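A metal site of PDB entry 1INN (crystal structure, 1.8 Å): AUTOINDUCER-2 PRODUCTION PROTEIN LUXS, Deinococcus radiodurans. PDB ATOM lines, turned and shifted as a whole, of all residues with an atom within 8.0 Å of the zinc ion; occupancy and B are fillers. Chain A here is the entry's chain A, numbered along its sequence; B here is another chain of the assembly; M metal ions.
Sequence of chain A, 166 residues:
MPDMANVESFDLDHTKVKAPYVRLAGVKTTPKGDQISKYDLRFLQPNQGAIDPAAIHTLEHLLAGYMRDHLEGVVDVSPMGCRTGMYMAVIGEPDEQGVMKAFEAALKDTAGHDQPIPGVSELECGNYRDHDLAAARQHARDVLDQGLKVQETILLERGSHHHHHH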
ATOM      1  N   HIS A  57       4.300 -29.422  21.808  1.00  0.00           N
ATOM      2  CA  HIS A  57       4.182 -28.014  21.423  1.00  0.00           C
ATOM      3  C   HIS A  57       5.598 -27.389  21.497  1.00  0.00           C
ATOM      4  O   HIS A  57       6.036 -26.636  20.607  1.00  0.00           O
ATOM      5  CB  HIS A  57       3.231 -27.330  22.396  1.00  0.00           C
ATOM      6  CG  HIS A  57       2.935 -25.893  22.069  1.00  0.00           C
ATOM      7  ND1 HIS A  57       2.300 -25.048  22.955  1.00  0.00           N
ATOM      8  CD2 HIS A  57       3.167 -25.170  20.951  1.00  0.00           C
ATOM      9  CE1 HIS A  57       2.150 -23.873  22.399  1.00  0.00           C
ATOM     10  NE2 HIS A  57       2.663 -23.913  21.183  1.00  0.00           N
ATOM     11  N   THR A  58       6.327 -27.723  22.554  1.00  0.00           N
ATOM     12  CA  THR A  58       7.676 -27.203  22.677  1.00  0.00           C
ATOM     13  C   THR A  58       8.586 -27.781  21.583  1.00  0.00           C
ATOM     14  O   THR A  58       9.437 -27.070  21.029  1.00  0.00           O
ATOM     15  CB  THR A  58       8.231 -27.512  24.086  1.00  0.00           C
ATOM     16  OG1 THR A  58       7.398 -26.858  25.055  1.00  0.00           O
ATOM     17  CG2 THR A  58       9.687 -27.020  24.233  1.00  0.00           C
ATOM     18  N   GLU A  60       7.743 -28.627  18.633  1.00  0.00           N
ATOM     19  CA  GLU A  60       7.393 -27.930  17.392  1.00  0.00           C
ATOM     20  C   GLU A  60       8.197 -26.630  17.303  1.00  0.00           C
ATOM     21  O   GLU A  60       8.831 -26.359  16.285  1.00  0.00           O
ATOM     22  CB  GLU A  60       5.882 -27.637  17.368  1.00  0.00           C
ATOM     23  CG  GLU A  60       5.403 -26.774  16.225  1.00  0.00           C
ATOM     24  CD  GLU A  60       4.008 -26.217  16.500  1.00  0.00           C
ATOM     25  OE1 GLU A  60       3.826 -25.526  17.541  1.00  0.00           O
ATOM     26  OE2 GLU A  60       3.091 -26.459  15.684  1.00  0.00           O
ATOM     27  N   HIS A  61       8.195 -25.844  18.380  1.00  0.00           N
ATOM     28  CA  HIS A  61       8.936 -24.585  18.416  1.00  0.00           C
ATOM     29  C   HIS A  61      10.461 -24.795  18.232  1.00  0.00           C
ATOM     30  O   HIS A  61      11.123 -24.064  17.490  1.00  0.00           O
ATOM     31  CB  HIS A  61       8.719 -23.865  19.741  1.00  0.00           C
ATOM     32  CG  HIS A  61       7.445 -23.091  19.808  1.00  0.00           C
ATOM     33  ND1 HIS A  61       7.409 -21.751  20.115  1.00  0.00           N
ATOM     34  CD2 HIS A  61       6.166 -23.466  19.564  1.00  0.00           C
ATOM     35  CE1 HIS A  61       6.165 -21.313  20.048  1.00  0.00           C
ATOM     36  NE2 HIS A  61       5.387 -22.336  19.712  1.00  0.00           N
ATOM     37  N   ILE A 117      12.602 -21.054  25.356  1.00  0.00           N
ATOM     38  CA  ILE A 117      11.994 -21.664  24.188  1.00  0.00           C
ATOM     39  C   ILE A 117      11.717 -20.534  23.227  1.00  0.00           C
ATOM     40  O   ILE A 117      11.055 -19.548  23.589  1.00  0.00           O
ATOM     41  CB  ILE A 117      10.653 -22.359  24.517  1.00  0.00           C
ATOM     42  CG1 ILE A 117      10.875 -23.498  25.509  1.00  0.00           C
ATOM     43  CG2 ILE A 117      10.030 -22.914  23.243  1.00  0.00           C
ATOM     44  CD1 ILE A 117       9.592 -23.900  26.258  1.00  0.00           C
ATOM     45  N   PRO A 118      12.213 -20.639  21.992  1.00  0.00           N
ATOM     46  CA  PRO A 118      11.964 -19.568  21.023  1.00  0.00           C
ATOM     47  C   PRO A 118      10.483 -19.415  20.654  1.00  0.00           C
ATOM     48  O   PRO A 118       9.756 -20.405  20.484  1.00  0.00           O
ATOM     49  CB  PRO A 118      12.829 -19.955  19.829  1.00  0.00           C
ATOM     50  CG  PRO A 118      12.909 -21.450  19.923  1.00  0.00           C
ATOM     51  CD  PRO A 118      13.075 -21.692  21.410  1.00  0.00           C
ATOM     52  N   GLY A 119      10.043 -18.161  20.551  1.00  0.00           N
ATOM     53  CA  GLY A 119       8.675 -17.865  20.164  1.00  0.00           C
ATOM     54  C   GLY A 119       7.611 -18.053  21.224  1.00  0.00           C
ATOM     55  O   GLY A 119       6.443 -18.202  20.896  1.00  0.00           O
ATOM     56  N   VAL A 120       8.003 -18.042  22.497  1.00  0.00           N
ATOM     57  CA  VAL A 120       7.036 -18.236  23.562  1.00  0.00           C
ATOM     58  C   VAL A 120       6.718 -16.952  24.315  1.00  0.00           C
ATOM     59  O   VAL A 120       7.536 -16.464  25.102  1.00  0.00           O
ATOM     60  CB  VAL A 120       7.517 -19.294  24.571  1.00  0.00           C
ATOM     61  CG1 VAL A 120       6.494 -19.420  25.702  1.00  0.00           C
ATOM     62  CG2 VAL A 120       7.694 -20.630  23.865  1.00  0.00           C
ATOM     63  N   SER A 121       5.523 -16.436  24.049  1.00  0.00           N
ATOM     64  CA  SER A 121       4.993 -15.228  24.674  1.00  0.00           C
ATOM     65  C   SER A 121       3.567 -15.135  24.125  1.00  0.00           C
ATOM     66  O   SER A 121       3.252 -15.779  23.116  1.00  0.00           O
ATOM     67  CB  SER A 121       5.802 -13.990  24.272  1.00  0.00           C
ATOM     68  OG  SER A 121       5.571 -13.632  22.916  1.00  0.00           O
ATOM     69  N   GLU A 124       3.702 -13.961  20.474  1.00  0.00           N
ATOM     70  CA  GLU A 124       4.230 -14.863  19.449  1.00  0.00           C
ATOM     71  C   GLU A 124       3.661 -16.274  19.384  1.00  0.00           C
ATOM     72  O   GLU A 124       3.994 -17.011  18.453  1.00  0.00           O
ATOM     73  CB  GLU A 124       5.748 -15.016  19.606  1.00  0.00           C
ATOM     74  CG  GLU A 124       6.546 -13.740  19.728  1.00  0.00           C
ATOM     75  CD  GLU A 124       7.876 -13.953  20.458  1.00  0.00           C
ATOM     76  OE1 GLU A 124       7.841 -14.309  21.660  1.00  0.00           O
ATOM     77  OE2 GLU A 124       8.943 -13.783  19.833  1.00  0.00           O
ATOM     78  N   CYS A 125       2.834 -16.669  20.339  1.00  0.00           N
ATOM     79  CA  CYS A 125       2.332 -18.036  20.365  1.00  0.00           C
ATOM     80  C   CYS A 125       0.895 -18.157  20.836  1.00  0.00           C
ATOM     81  O   CYS A 125       0.514 -17.567  21.853  1.00  0.00           O
ATOM     82  CB  CYS A 125       3.296 -18.862  21.230  1.00  0.00           C
ATOM     83  SG  CYS A 125       2.676 -20.416  21.899  1.00  0.00           S
ATOM     84  N   GLY A 126       0.101 -18.925  20.096  1.00  0.00           N
ATOM     85  CA  GLY A 126      -1.311 -19.128  20.389  1.00  0.00           C
ATOM     86  C   GLY A 126      -1.733 -19.800  21.683  1.00  0.00           C
ATOM     87  O   GLY A 126      -2.922 -19.775  22.010  1.00  0.00           O
ATOM     88  N   ASN A 127      -0.791 -20.402  22.421  1.00  0.00           N
ATOM     89  CA  ASN A 127      -1.077 -21.078  23.687  1.00  0.00           C
ATOM     90  C   ASN A 127       0.248 -21.076  24.468  1.00  0.00           C
ATOM     91  O   ASN A 127       0.747 -22.123  24.876  1.00  0.00           O
ATOM     92  CB  ASN A 127      -1.555 -22.518  23.422  1.00  0.00           C
ATOM     93  CG  ASN A 127      -2.256 -23.145  24.619  1.00  0.00           C
ATOM     94  OD1 ASN A 127      -2.419 -22.509  25.666  1.00  0.00           O
ATOM     95  ND2 ASN A 127      -2.695 -24.400  24.459  1.00  0.00           N
ATOM     96  N   TYR A 128       0.803 -19.873  24.684  1.00  0.00           N
ATOM     97  CA  TYR A 128       2.107 -19.692  25.321  1.00  0.00           C
ATOM     98  C   TYR A 128       2.351 -20.340  26.686  1.00  0.00           C
ATOM     99  O   TYR A 128       3.506 -20.580  27.062  1.00  0.00           O
ATOM    100  CB  TYR A 128       2.441 -18.190  25.379  1.00  0.00           C
ATOM    101  CG  TYR A 128       2.001 -17.488  26.649  1.00  0.00           C
ATOM    102  CD1 TYR A 128       2.889 -17.338  27.735  1.00  0.00           C
ATOM    103  CD2 TYR A 128       0.722 -16.965  26.774  1.00  0.00           C
ATOM    104  CE1 TYR A 128       2.487 -16.675  28.907  1.00  0.00           C
ATOM    105  CE2 TYR A 128       0.309 -16.299  27.939  1.00  0.00           C
ATOM    106  CZ  TYR A 128       1.193 -16.168  28.999  1.00  0.00           C
ATOM    107  OH  TYR A 128       0.775 -15.524  30.153  1.00  0.00           O
ATOM    108  N   ARG A 129       1.296 -20.648  27.425  1.00  0.00           N
ATOM    109  CA  ARG A 129       1.507 -21.282  28.725  1.00  0.00           C
ATOM    110  C   ARG A 129       1.638 -22.807  28.601  1.00  0.00           C
ATOM    111  O   ARG A 129       2.149 -23.465  29.501  1.00  0.00           O
ATOM    112  CB  ARG A 129       0.347 -20.922  29.671  1.00  0.00           C
ATOM    113  CG  ARG A 129       0.387 -19.453  30.121  1.00  0.00           C
ATOM    114  CD  ARG A 129      -0.928 -18.988  30.758  1.00  0.00           C
ATOM    115  NE  ARG A 129      -2.015 -18.899  29.779  1.00  0.00           N
ATOM    116  CZ  ARG A 129      -3.139 -18.220  29.970  1.00  0.00           C
ATOM    117  NH1 ARG A 129      -3.350 -17.574  31.110  1.00  0.00           N
ATOM    118  NH2 ARG A 129      -4.062 -18.185  29.015  1.00  0.00           N
ATOM    119  N   ASP A 130       1.217 -23.363  27.463  1.00  0.00           N
ATOM    120  CA  ASP A 130       1.271 -24.817  27.268  1.00  0.00           C
ATOM    121  C   ASP A 130       2.571 -25.351  26.660  1.00  0.00           C
ATOM    122  O   ASP A 130       2.596 -25.848  25.534  1.00  0.00           O
ATOM    123  CB  ASP A 130       0.074 -25.261  26.420  1.00  0.00           C
ATOM    124  CG  ASP A 130      -0.165 -26.754  26.507  1.00  0.00           C
ATOM    125  OD1 ASP A 130      -0.154 -27.287  27.631  1.00  0.00           O
ATOM    126  OD2 ASP A 130      -0.392 -27.395  25.454  1.00  0.00           O
ATOM    127  N   HIS A 131       3.645 -25.248  27.449  1.00  0.00           N
ATOM    128  CA  HIS A 131       4.968 -25.709  27.050  1.00  0.00           C
ATOM    129  C   HIS A 131       5.619 -26.559  28.127  1.00  0.00           C
ATOM    130  O   HIS A 131       5.260 -26.454  29.322  1.00  0.00           O
ATOM    131  CB  HIS A 131       5.876 -24.498  26.737  1.00  0.00           C
ATOM    132  CG  HIS A 131       5.633 -23.899  25.385  1.00  0.00           C
ATOM    133  ND1 HIS A 131       6.084 -24.485  24.222  1.00  0.00           N
ATOM    134  CD2 HIS A 131       4.944 -22.789  25.011  1.00  0.00           C
ATOM    135  CE1 HIS A 131       5.684 -23.756  23.184  1.00  0.00           C
ATOM    136  NE2 HIS A 131       4.983 -22.733  23.643  1.00  0.00           N
ATOM    137  N   HIS B  14      -0.159 -12.306  17.836  1.00  0.00           N
ATOM    138  CA  HIS B  14      -1.347 -13.098  18.165  1.00  0.00           C
ATOM    139  C   HIS B  14      -2.424 -12.381  18.963  1.00  0.00           C
ATOM    140  O   HIS B  14      -3.534 -12.900  19.115  1.00  0.00           O
ATOM    141  CB  HIS B  14      -0.944 -14.374  18.908  1.00  0.00           C
ATOM    142  CG  HIS B  14      -0.177 -15.345  18.060  1.00  0.00           C
ATOM    143  ND1 HIS B  14       1.008 -15.013  17.443  1.00  0.00           N
ATOM    144  CD2 HIS B  14      -0.425 -16.639  17.756  1.00  0.00           C
ATOM    145  CE1 HIS B  14       1.464 -16.070  16.789  1.00  0.00           C
ATOM    146  NE2 HIS B  14       0.611 -17.070  16.955  1.00  0.00           N
ATOM    147  N   ARG B  42      -7.415 -20.677  11.647  1.00  0.00           N
ATOM    148  CA  ARG B  42      -7.681 -20.426  13.053  1.00  0.00           C
ATOM    149  C   ARG B  42      -9.109 -20.711  13.518  1.00  0.00           C
ATOM    150  O   ARG B  42     -10.039 -20.100  13.028  1.00  0.00           O
ATOM    151  CB  ARG B  42      -7.370 -18.956  13.334  1.00  0.00           C
ATOM    152  CG  ARG B  42      -6.696 -18.707  14.631  1.00  0.00           C
ATOM    153  CD  ARG B  42      -5.197 -18.666  14.330  1.00  0.00           C
ATOM    154  NE  ARG B  42      -4.528 -19.210  15.461  1.00  0.00           N
ATOM    155  CZ  ARG B  42      -3.214 -19.267  15.641  1.00  0.00           C
ATOM    156  NH1 ARG B  42      -2.807 -19.818  16.768  1.00  0.00           N
ATOM    157  NH2 ARG B  42      -2.348 -18.813  14.736  1.00  0.00           N
ATOM    158  N   ASN B  47      -4.688 -17.919  22.834  1.00  0.00           N
ATOM    159  CA  ASN B  47      -4.616 -17.827  24.293  1.00  0.00           C
ATOM    160  C   ASN B  47      -5.887 -17.592  25.088  1.00  0.00           C
ATOM    161  O   ASN B  47      -5.844 -16.991  26.165  1.00  0.00           O
ATOM    162  CB  ASN B  47      -3.562 -16.783  24.680  1.00  0.00           C
ATOM    163  CG  ASN B  47      -2.172 -17.168  24.198  1.00  0.00           C
ATOM    164  OD1 ASN B  47      -1.623 -18.172  24.645  1.00  0.00           O
ATOM    165  ND2 ASN B  47      -1.617 -16.396  23.290  1.00  0.00           N
ATOM    166  N   MET B  80      -2.038 -27.429  14.880  1.00  0.00           N
ATOM    167  CA  MET B  80      -0.949 -26.589  15.343  1.00  0.00           C
ATOM    168  C   MET B  80      -0.607 -27.022  16.759  1.00  0.00           C
ATOM    169  O   MET B  80      -1.473 -27.495  17.503  1.00  0.00           O
ATOM    170  CB  MET B  80      -1.359 -25.100  15.363  1.00  0.00           C
ATOM    171  CG  MET B  80      -1.757 -24.534  14.016  1.00  0.00           C
ATOM    172  SD  MET B  80      -2.166 -22.609  14.189  1.00  0.00           S
ATOM    173  CE  MET B  80      -3.658 -22.695  15.317  1.00  0.00           C
ATOM    174  N   GLY B  81       0.657 -26.855  17.154  1.00  0.00           N
ATOM    175  CA  GLY B  81       1.061 -27.220  18.492  1.00  0.00           C
ATOM    176  C   GLY B  81       0.271 -26.456  19.555  1.00  0.00           C
ATOM    177  O   GLY B  81       0.054 -26.982  20.651  1.00  0.00           O
ATOM    178  N   CYS B  82      -0.148 -25.237  19.240  1.00  0.00           N
ATOM    179  CA  CYS B  82      -0.910 -24.412  20.185  1.00  0.00           C
ATOM    180  C   CYS B  82      -2.380 -24.847  20.284  1.00  0.00           C
ATOM    181  O   CYS B  82      -3.104 -24.401  21.160  1.00  0.00           O
ATOM    182  CB  CYS B  82      -0.829 -22.933  19.826  1.00  0.00           C
ATOM    183  SG  CYS B  82      -1.266 -22.513  18.121  1.00  0.00           S
ATOM    184  N   ARG B  83      -2.790 -25.746  19.390  1.00  0.00           N
ATOM    185  CA  ARG B  83      -4.133 -26.318  19.387  1.00  0.00           C
ATOM    186  C   ARG B  83      -5.310 -25.346  19.294  1.00  0.00           C
ATOM    187  O   ARG B  83      -6.387 -25.614  19.815  1.00  0.00           O
ATOM    188  CB  ARG B  83      -4.278 -27.249  20.619  1.00  0.00           C
ATOM    189  CG  ARG B  83      -3.426 -28.558  20.467  1.00  0.00           C
ATOM    190  CD  ARG B  83      -3.111 -29.272  21.782  1.00  0.00           C
ATOM    191  NE  ARG B  83      -4.253 -29.254  22.664  1.00  0.00           N
ATOM    192  CZ  ARG B  83      -4.294 -28.738  23.886  1.00  0.00           C
ATOM    193  NH1 ARG B  83      -5.418 -28.790  24.563  1.00  0.00           N
ATOM    194  NH2 ARG B  83      -3.218 -28.193  24.434  1.00  0.00           N
HETATM  195 ZN    ZN M   1       3.284 -22.064  20.277  1.00  0.00          ZN
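The zinc ion is bound by a ring nitrogen (NE2) of His 57, a ring nitrogen (NE2) of His 61 and the side-chain sulfur of Cys 125. The zinc ion has three donor atoms within binding distance.
Merely in contact with the zinc ion: His 131 (3.8 Å). Within 4 Å of the zinc ion: His 57, His 61, Cys 125 and His 131. The nearest printed residue that does not touch the zinc ion is Cys 82 of chain B (4.2 Å).
A ring nitrogen (ND1) of His 57 is in hydrogen-bond range of the backbone carbonyl oxygen of Asp 130. A ring nitrogen (ND1) of His 61 is in hydrogen-bond range of the backbone carbonyl oxygen (O) of Pro 118 (2.7 Å). SG of Cys 125 sits close to NE2 of His 131, 3.7 Å away. The backbone NH (N) of Asn 127 sits close to the side-chain sulfur (SG) of Cys 125 (3.5 Å). The backbone NH (N) of Tyr 128 lies close to the side-chain sulfur (SG) of Cys 125 (3.4 Å). The backbone carbonyl oxygen (O) of Cys 125 sits at hydrogen-bond distance from the side-chain amide nitrogen (ND2) of Asn 47 of chain B, at 2.8 Å. ND1 of His 131 sits at hydrogen-bond distance from OG1 of Thr 58 (2.8 Å).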
